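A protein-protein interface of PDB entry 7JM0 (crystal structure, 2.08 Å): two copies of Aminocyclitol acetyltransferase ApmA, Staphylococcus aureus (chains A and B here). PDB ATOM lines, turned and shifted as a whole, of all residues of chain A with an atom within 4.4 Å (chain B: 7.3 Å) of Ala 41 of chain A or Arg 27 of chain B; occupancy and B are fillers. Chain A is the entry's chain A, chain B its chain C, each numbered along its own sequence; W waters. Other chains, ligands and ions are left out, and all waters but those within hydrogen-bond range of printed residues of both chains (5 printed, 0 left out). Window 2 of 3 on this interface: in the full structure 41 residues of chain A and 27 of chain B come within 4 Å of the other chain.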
ATOM      1  N   ALA A  20      -8.699 -11.854  34.515  1.00  0.00           N
ATOM      2  CA  ALA A  20      -8.260 -10.530  34.093  1.00  0.00           C
ATOM      3  C   ALA A  20      -7.589 -10.669  32.731  1.00  0.00           C
ATOM      4  O   ALA A  20      -6.530 -11.293  32.615  1.00  0.00           O
ATOM      5  CB  ALA A  20      -7.314  -9.914  35.122  1.00  0.00           C
ATOM      6  N   VAL A  21      -8.212 -10.098  31.706  1.00  0.00           N
ATOM      7  CA  VAL A  21      -7.720 -10.230  30.339  1.00  0.00           C
ATOM      8  C   VAL A  21      -6.612  -9.209  30.112  1.00  0.00           C
ATOM      9  O   VAL A  21      -6.845  -7.998  30.188  1.00  0.00           O
ATOM     10  CB  VAL A  21      -8.856 -10.050  29.322  1.00  0.00           C
ATOM     11  CG1 VAL A  21      -8.333 -10.231  27.906  1.00  0.00           C
ATOM     12  CG2 VAL A  21      -9.988 -11.028  29.608  1.00  0.00           C
ATOM     13  N   TRP A  22      -5.405  -9.700  29.831  1.00  0.00           N
ATOM     14  CA  TRP A  22      -4.236  -8.863  29.563  1.00  0.00           C
ATOM     15  C   TRP A  22      -4.000  -8.882  28.055  1.00  0.00           C
ATOM     16  O   TRP A  22      -3.299  -9.746  27.528  1.00  0.00           O
ATOM     17  CB  TRP A  22      -3.025  -9.378  30.334  1.00  0.00           C
ATOM     18  CG  TRP A  22      -1.909  -8.383  30.496  1.00  0.00           C
ATOM     19  CD1 TRP A  22      -0.969  -8.040  29.561  1.00  0.00           C
ATOM     20  CD2 TRP A  22      -1.603  -7.620  31.670  1.00  0.00           C
ATOM     21  NE1 TRP A  22      -0.105  -7.105  30.081  1.00  0.00           N
ATOM     22  CE2 TRP A  22      -0.472  -6.829  31.372  1.00  0.00           C
ATOM     23  CE3 TRP A  22      -2.176  -7.525  32.941  1.00  0.00           C
ATOM     24  CZ2 TRP A  22       0.092  -5.955  32.299  1.00  0.00           C
ATOM     25  CZ3 TRP A  22      -1.612  -6.657  33.861  1.00  0.00           C
ATOM     26  CH2 TRP A  22      -0.491  -5.884  33.535  1.00  0.00           C
ATOM     27  N   GLY A  23      -4.600  -7.925  27.357  1.00  0.00           N
ATOM     28  CA  GLY A  23      -4.505  -7.837  25.916  1.00  0.00           C
ATOM     29  C   GLY A  23      -5.865  -7.653  25.278  1.00  0.00           C
ATOM     30  O   GLY A  23      -6.902  -7.654  25.937  1.00  0.00           O
ATOM     31  N   HIS A  39     -12.847  -9.402  33.014  1.00  0.00           N
ATOM     32  CA  HIS A  39     -12.745  -7.976  32.743  1.00  0.00           C
ATOM     33  C   HIS A  39     -11.373  -7.700  32.151  1.00  0.00           C
ATOM     34  O   HIS A  39     -10.445  -8.501  32.293  1.00  0.00           O
ATOM     35  CB  HIS A  39     -12.948  -7.137  34.016  1.00  0.00           C
ATOM     36  CG  HIS A  39     -13.260  -5.694  33.756  1.00  0.00           C
ATOM     37  ND1 HIS A  39     -12.290  -4.763  33.443  1.00  0.00           N
ATOM     38  CD2 HIS A  39     -14.432  -5.018  33.784  1.00  0.00           C
ATOM     39  CE1 HIS A  39     -12.855  -3.580  33.276  1.00  0.00           C
ATOM     40  NE2 HIS A  39     -14.154  -3.706  33.480  1.00  0.00           N
ATOM     41  N   THR A  40     -11.261  -6.563  31.469  1.00  0.00           N
ATOM     42  CA  THR A  40      -9.957  -6.027  31.111  1.00  0.00           C
ATOM     43  C   THR A  40      -9.083  -5.931  32.355  1.00  0.00           C
ATOM     44  O   THR A  40      -9.528  -5.460  33.405  1.00  0.00           O
ATOM     45  CB  THR A  40     -10.113  -4.645  30.470  1.00  0.00           C
ATOM     46  OG1 THR A  40     -10.999  -4.731  29.346  1.00  0.00           O
ATOM     47  CG2 THR A  40      -8.766  -4.108  30.015  1.00  0.00           C
ATOM     48  N   ALA A  41      -7.841  -6.395  32.237  1.00  0.00           N
ATOM     49  CA  ALA A  41      -6.922  -6.348  33.365  1.00  0.00           C
ATOM     50  C   ALA A  41      -6.446  -4.922  33.607  1.00  0.00           C
ATOM     51  O   ALA A  41      -6.048  -4.220  32.671  1.00  0.00           O
ATOM     52  CB  ALA A  41      -5.726  -7.266  33.115  1.00  0.00           C
ATOM     53  N   ASP A  42      -6.496  -4.493  34.866  1.00  0.00           N
ATOM     54  CA  ASP A  42      -5.908  -3.225  35.275  1.00  0.00           C
ATOM     55  C   ASP A  42      -4.985  -3.480  36.459  1.00  0.00           C
ATOM     56  O   ASP A  42      -3.826  -3.864  36.273  1.00  0.00           O
ATOM     57  CB  ASP A  42      -6.995  -2.201  35.622  1.00  0.00           C
ATOM     58  CG  ASP A  42      -6.439  -0.801  35.833  1.00  0.00           C
ATOM     59  OD1 ASP A  42      -5.202  -0.632  35.787  1.00  0.00           O
ATOM     60  OD2 ASP A  42      -7.236   0.137  36.050  1.00  0.00           O
ATOM     61  N   VAL A  44      -4.278  -5.994  39.466  1.00  0.00           N
ATOM     62  CA  VAL A  44      -4.594  -7.396  39.699  1.00  0.00           C
ATOM     63  C   VAL A  44      -3.836  -7.906  40.916  1.00  0.00           C
ATOM     64  O   VAL A  44      -2.739  -7.438  41.238  1.00  0.00           O
ATOM     65  CB  VAL A  44      -4.280  -8.270  38.464  1.00  0.00           C
ATOM     66  CG1 VAL A  44      -5.219  -7.922  37.316  1.00  0.00           C
ATOM     67  CG2 VAL A  44      -2.825  -8.098  38.041  1.00  0.00           C
ATOM     68  N   ASP A  58       1.490 -10.356  24.611  1.00  0.00           N
ATOM     69  CA  ASP A  58       0.848  -9.851  25.821  1.00  0.00           C
ATOM     70  C   ASP A  58       1.480 -10.449  27.069  1.00  0.00           C
ATOM     71  O   ASP A  58       1.685  -9.747  28.065  1.00  0.00           O
ATOM     72  CB  ASP A  58      -0.651 -10.161  25.792  1.00  0.00           C
ATOM     73  CG  ASP A  58      -1.384  -9.425  24.687  1.00  0.00           C
ATOM     74  OD1 ASP A  58      -1.032  -8.262  24.401  1.00  0.00           O
ATOM     75  OD2 ASP A  58      -2.323 -10.012  24.107  1.00  0.00           O
ATOM     76  N   ASP A  61       4.570  -8.687  27.955  1.00  0.00           N
ATOM     77  CA  ASP A  61       4.298  -7.433  28.647  1.00  0.00           C
ATOM     78  C   ASP A  61       3.896  -7.680  30.097  1.00  0.00           C
ATOM     79  O   ASP A  61       4.322  -6.945  30.998  1.00  0.00           O
ATOM     80  CB  ASP A  61       3.207  -6.657  27.912  1.00  0.00           C
ATOM     81  CG  ASP A  61       2.887  -5.337  28.578  1.00  0.00           C
ATOM     82  OD1 ASP A  61       3.625  -4.359  28.338  1.00  0.00           O
ATOM     83  OD2 ASP A  61       1.903  -5.280  29.347  1.00  0.00           O
ATOM     84  N   PRO B  25      -4.140  -0.722  18.974  1.00  0.00           N
ATOM     85  CA  PRO B  25      -3.006  -0.749  19.903  1.00  0.00           C
ATOM     86  C   PRO B  25      -2.904  -2.084  20.625  1.00  0.00           C
ATOM     87  O   PRO B  25      -3.862  -2.856  20.711  1.00  0.00           O
ATOM     88  CB  PRO B  25      -3.322   0.389  20.877  1.00  0.00           C
ATOM     89  CG  PRO B  25      -4.815   0.480  20.860  1.00  0.00           C
ATOM     90  CD  PRO B  25      -5.236   0.137  19.455  1.00  0.00           C
ATOM     91  N   THR B  26      -1.709  -2.350  21.143  1.00  0.00           N
ATOM     92  CA  THR B  26      -1.424  -3.548  21.918  1.00  0.00           C
ATOM     93  C   THR B  26      -0.875  -3.153  23.283  1.00  0.00           C
ATOM     94  O   THR B  26      -0.477  -2.008  23.512  1.00  0.00           O
ATOM     95  CB  THR B  26      -0.421  -4.456  21.198  1.00  0.00           C
ATOM     96  OG1 THR B  26       0.879  -3.857  21.242  1.00  0.00           O
ATOM     97  CG2 THR B  26      -0.828  -4.672  19.743  1.00  0.00           C
ATOM     98  N   ARG B  27      -0.855  -4.126  24.199  1.00  0.00           N
ATOM     99  CA  ARG B  27      -0.259  -3.894  25.511  1.00  0.00           C
ATOM    100  C   ARG B  27       1.212  -3.508  25.391  1.00  0.00           C
ATOM    101  O   ARG B  27       1.681  -2.598  26.084  1.00  0.00           O
ATOM    102  CB  ARG B  27      -0.415  -5.137  26.384  1.00  0.00           C
ATOM    103  CG  ARG B  27      -1.807  -5.305  26.960  1.00  0.00           C
ATOM    104  CD  ARG B  27      -1.963  -4.529  28.259  1.00  0.00           C
ATOM    105  NE  ARG B  27      -3.283  -4.727  28.847  1.00  0.00           N
ATOM    106  CZ  ARG B  27      -3.579  -4.497  30.122  1.00  0.00           C
ATOM    107  NH1 ARG B  27      -2.645  -4.061  30.955  1.00  0.00           N
ATOM    108  NH2 ARG B  27      -4.810  -4.706  30.562  1.00  0.00           N
ATOM    109  N   ARG B  28       1.954  -4.185  24.512  1.00  0.00           N
ATOM    110  CA  ARG B  28       3.365  -3.856  24.330  1.00  0.00           C
ATOM    111  C   ARG B  28       3.535  -2.441  23.792  1.00  0.00           C
ATOM    112  O   ARG B  28       4.471  -1.732  24.178  1.00  0.00           O
ATOM    113  CB  ARG B  28       4.024  -4.870  23.393  1.00  0.00           C
ATOM    114  CG  ARG B  28       4.440  -6.168  24.067  1.00  0.00           C
ATOM    115  CD  ARG B  28       5.831  -6.045  24.673  1.00  0.00           C
ATOM    116  NE  ARG B  28       6.878  -6.022  23.654  1.00  0.00           N
ATOM    117  CZ  ARG B  28       8.139  -5.667  23.886  1.00  0.00           C
ATOM    118  NH1 ARG B  28       8.516  -5.301  25.104  1.00  0.00           N
ATOM    119  NH2 ARG B  28       9.024  -5.676  22.898  1.00  0.00           N
ATOM    120  N   LEU B  29       2.634  -2.012  22.906  1.00  0.00           N
ATOM    121  CA  LEU B  29       2.722  -0.666  22.349  1.00  0.00           C
ATOM    122  C   LEU B  29       2.464   0.391  23.414  1.00  0.00           C
ATOM    123  O   LEU B  29       3.234   1.350  23.550  1.00  0.00           O
ATOM    124  CB  LEU B  29       1.734  -0.515  21.190  1.00  0.00           C
ATOM    125  CG  LEU B  29       1.588   0.893  20.604  1.00  0.00           C
ATOM    126  CD1 LEU B  29       2.879   1.336  19.933  1.00  0.00           C
ATOM    127  CD2 LEU B  29       0.425   0.950  19.627  1.00  0.00           C
ATOM    128  N   LEU B  30       1.383   0.231  24.183  1.00  0.00           N
ATOM    129  CA  LEU B  30       1.054   1.218  25.207  1.00  0.00           C
ATOM    130  C   LEU B  30       2.144   1.310  26.267  1.00  0.00           C
ATOM    131  O   LEU B  30       2.392   2.392  26.811  1.00  0.00           O
ATOM    132  CB  LEU B  30      -0.293   0.880  25.847  1.00  0.00           C
ATOM    133  CG  LEU B  30      -1.527   1.010  24.947  1.00  0.00           C
ATOM    134  CD1 LEU B  30      -2.809   0.831  25.754  1.00  0.00           C
ATOM    135  CD2 LEU B  30      -1.534   2.349  24.221  1.00  0.00           C
ATOM    136  N   ARG B  31       2.807   0.191  26.570  1.00  0.00           N
ATOM    137  CA  ARG B  31       3.953   0.233  27.473  1.00  0.00           C
ATOM    138  C   ARG B  31       5.107   1.013  26.854  1.00  0.00           C
ATOM    139  O   ARG B  31       5.827   1.732  27.556  1.00  0.00           O
ATOM    140  CB  ARG B  31       4.392  -1.188  27.825  1.00  0.00           C
ATOM    141  CG  ARG B  31       5.583  -1.270  28.772  1.00  0.00           C
ATOM    142  CD  ARG B  31       5.137  -1.364  30.221  1.00  0.00           C
ATOM    143  NE  ARG B  31       4.417  -2.609  30.483  1.00  0.00           N
ATOM    144  CZ  ARG B  31       3.840  -2.909  31.642  1.00  0.00           C
ATOM    145  NH1 ARG B  31       3.895  -2.054  32.656  1.00  0.00           N
ATOM    146  NH2 ARG B  31       3.206  -4.063  31.786  1.00  0.00           N
ATOM    147  N   ALA B  32       5.289   0.893  25.538  1.00  0.00           N
ATOM    148  CA  ALA B  32       6.381   1.597  24.876  1.00  0.00           C
ATOM    149  C   ALA B  32       6.094   3.086  24.731  1.00  0.00           C
ATOM    150  O   ALA B  32       7.031   3.889  24.653  1.00  0.00           O
ATOM    151  CB  ALA B  32       6.653   0.974  23.507  1.00  0.00           C
ATOM    152  N   LEU B  33       4.820   3.473  24.701  1.00  0.00           N
ATOM    153  CA  LEU B  33       4.429   4.859  24.480  1.00  0.00           C
ATOM    154  C   LEU B  33       4.220   5.643  25.768  1.00  0.00           C
ATOM    155  O   LEU B  33       3.955   6.849  25.702  1.00  0.00           O
ATOM    156  CB  LEU B  33       3.148   4.918  23.642  1.00  0.00           C
ATOM    157  CG  LEU B  33       3.260   4.474  22.183  1.00  0.00           C
ATOM    158  CD1 LEU B  33       1.915   4.594  21.486  1.00  0.00           C
ATOM    159  CD2 LEU B  33       4.326   5.288  21.456  1.00  0.00           C
ATOM    160  N   PHE B  80       5.627  -0.527  14.808  1.00  0.00           N
ATOM    161  CA  PHE B  80       5.982  -1.024  16.133  1.00  0.00           C
ATOM    162  C   PHE B  80       6.356  -2.501  16.097  1.00  0.00           C
ATOM    163  O   PHE B  80       7.352  -2.904  16.708  1.00  0.00           O
ATOM    164  CB  PHE B  80       4.843  -0.788  17.123  1.00  0.00           C
ATOM    165  CG  PHE B  80       5.151  -1.275  18.508  1.00  0.00           C
ATOM    166  CD1 PHE B  80       6.208  -0.731  19.223  1.00  0.00           C
ATOM    167  CD2 PHE B  80       4.405  -2.287  19.087  1.00  0.00           C
ATOM    168  CE1 PHE B  80       6.504  -1.179  20.499  1.00  0.00           C
ATOM    169  CE2 PHE B  80       4.697  -2.739  20.360  1.00  0.00           C
ATOM    170  CZ  PHE B  80       5.746  -2.186  21.068  1.00  0.00           C
HETATM  171  O   HOH W   1       1.002  -6.910  23.560  1.00  0.00           O
HETATM  172  O   HOH W   2       0.656  -3.244  29.862  1.00  0.00           O
HETATM  173  O   HOH W   3      -2.881  -3.328  33.604  1.00  0.00           O
HETATM  174  O   HOH W   4      -2.511  -6.456  23.412  1.00  0.00           O
HETATM  175  O   HOH W   5      -6.417  -5.699  28.106  1.00  0.00           O
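The backbone carbonyl oxygen (O) of Ala 41 of chain A sits at hydrogen-bond distance from the guanidinium group (NH2) of Arg 27 of chain B. NE of Arg 31 of chain B is in salt-bridge range of OD1 of Asp 61 of chain A, 2.9 Å away. The side-chain carboxylate (OD1) of Asp 61 of chain A sits close to the backbone carbonyl oxygen (O) of Arg 27 of chain B, at 3.5 Å.
The backbone NH (N) of Val 21 of chain A sits at hydrogen-bond distance from the backbone carbonyl oxygen (O) of His 39 of chain A. The backbone carbonyl oxygen (O) of Val 21 of chain A sits at hydrogen-bond distance from the backbone NH (N) of Ala 41 of chain A, 2.8 Å away. The side-chain carboxylate (OD2) of Asp 61 of chain A sits at hydrogen-bond distance from the indole nitrogen (NE1) of Trp 22 of chain A (2.8 Å).
Among the printed residues, pairs that only touch across the chains: Trp 22 of chain A with Arg 27 of chain B (3.5 Å), Trp 22 of chain A with Arg 31 of chain B (3.7 Å), Asp 58 of chain A with Arg 27 of chain B (3.8 Å), Gly 23 of chain A with Arg 27 of chain B (3.8 Å) and Val 21 of chain A with Arg 27 of chain B (3.9 Å).
Of the printed residues of chain B, Val 21 of chain A touches Arg 27 (3.9 Å). Of the printed residues of chain B, Gly 23 of chain A touches Arg 27. Of chain B, only Arg 27 (2.5 Å) comes within 4 Å of Ala 41 of chain A. Val 44 of chain A touches none of the printed residues of chain B. Of the printed residues of chain B, Asp 58 of chain A touches Arg 27. Of the printed residues of chain B, Asp 61 of chain A touches Arg 27 and Arg 31. Arg 27 of chain B touches six residues of chain A. Leu 30 of chain B touches none of the printed residues of chain A. Of the printed residues of chain A, Arg 31 of chain B touches Trp 22 (3.7 Å) and Asp 61 (2.9 Å). The nearest printed residue of chain B that does not touch Ala 41 of chain A is Leu 30 of chain B (9.2 Å).
Printed residues of chain B that touch a printed residue of chain A: Arg 27 and Arg 31. Of the 11 printed residues of chain A, 6 touch a printed residue of chain B. Hydrophobic or aromatic side chains of chain A that line the printed part of chain B: Trp 22 and Ala 41. Among the printed residues, 8 pairs touch across the chains. Among the printed residues, Asp or Glu carboxylates within 4 Å of a Lys or Arg side-chain nitrogen of the other chain: Asp 61 of chain A with Arg 31 of chain B (2.9 Å).
No position is printed for both chains.
Water W2 bridges OD2 of Asp 61 of chain A (2.4 Å) and NH2 of Arg 31 of chain B (3.3 Å). Water W4 bridges the side-chain carboxylate of Asp 58 of chain A (2.5 Å) and the backbone NH of Arg 27 of chain B (3.0 Å). Water W1 lies within hydrogen-bond range of the side-chain carboxylate of Asp 58 of chain A (2.6 Å), the backbone NH of Arg 28 of chain B (3.0 Å) and the backbone NH of Arg 27 of chain B (3.4 Å). Water W3 lies within hydrogen-bond range of the guanidinium group of Arg 27 of chain B (2.8 Å), the backbone carbonyl oxygen of Asp 42 of chain A (2.9 Å) and the backbone carbonyl oxygen of Ala 41 of chain A (3.4 Å). Water W5 lies within hydrogen-bond range of O of Gly 23 of chain A, NH2 of Arg 27 of chain B and O of Val 21 of chain A.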
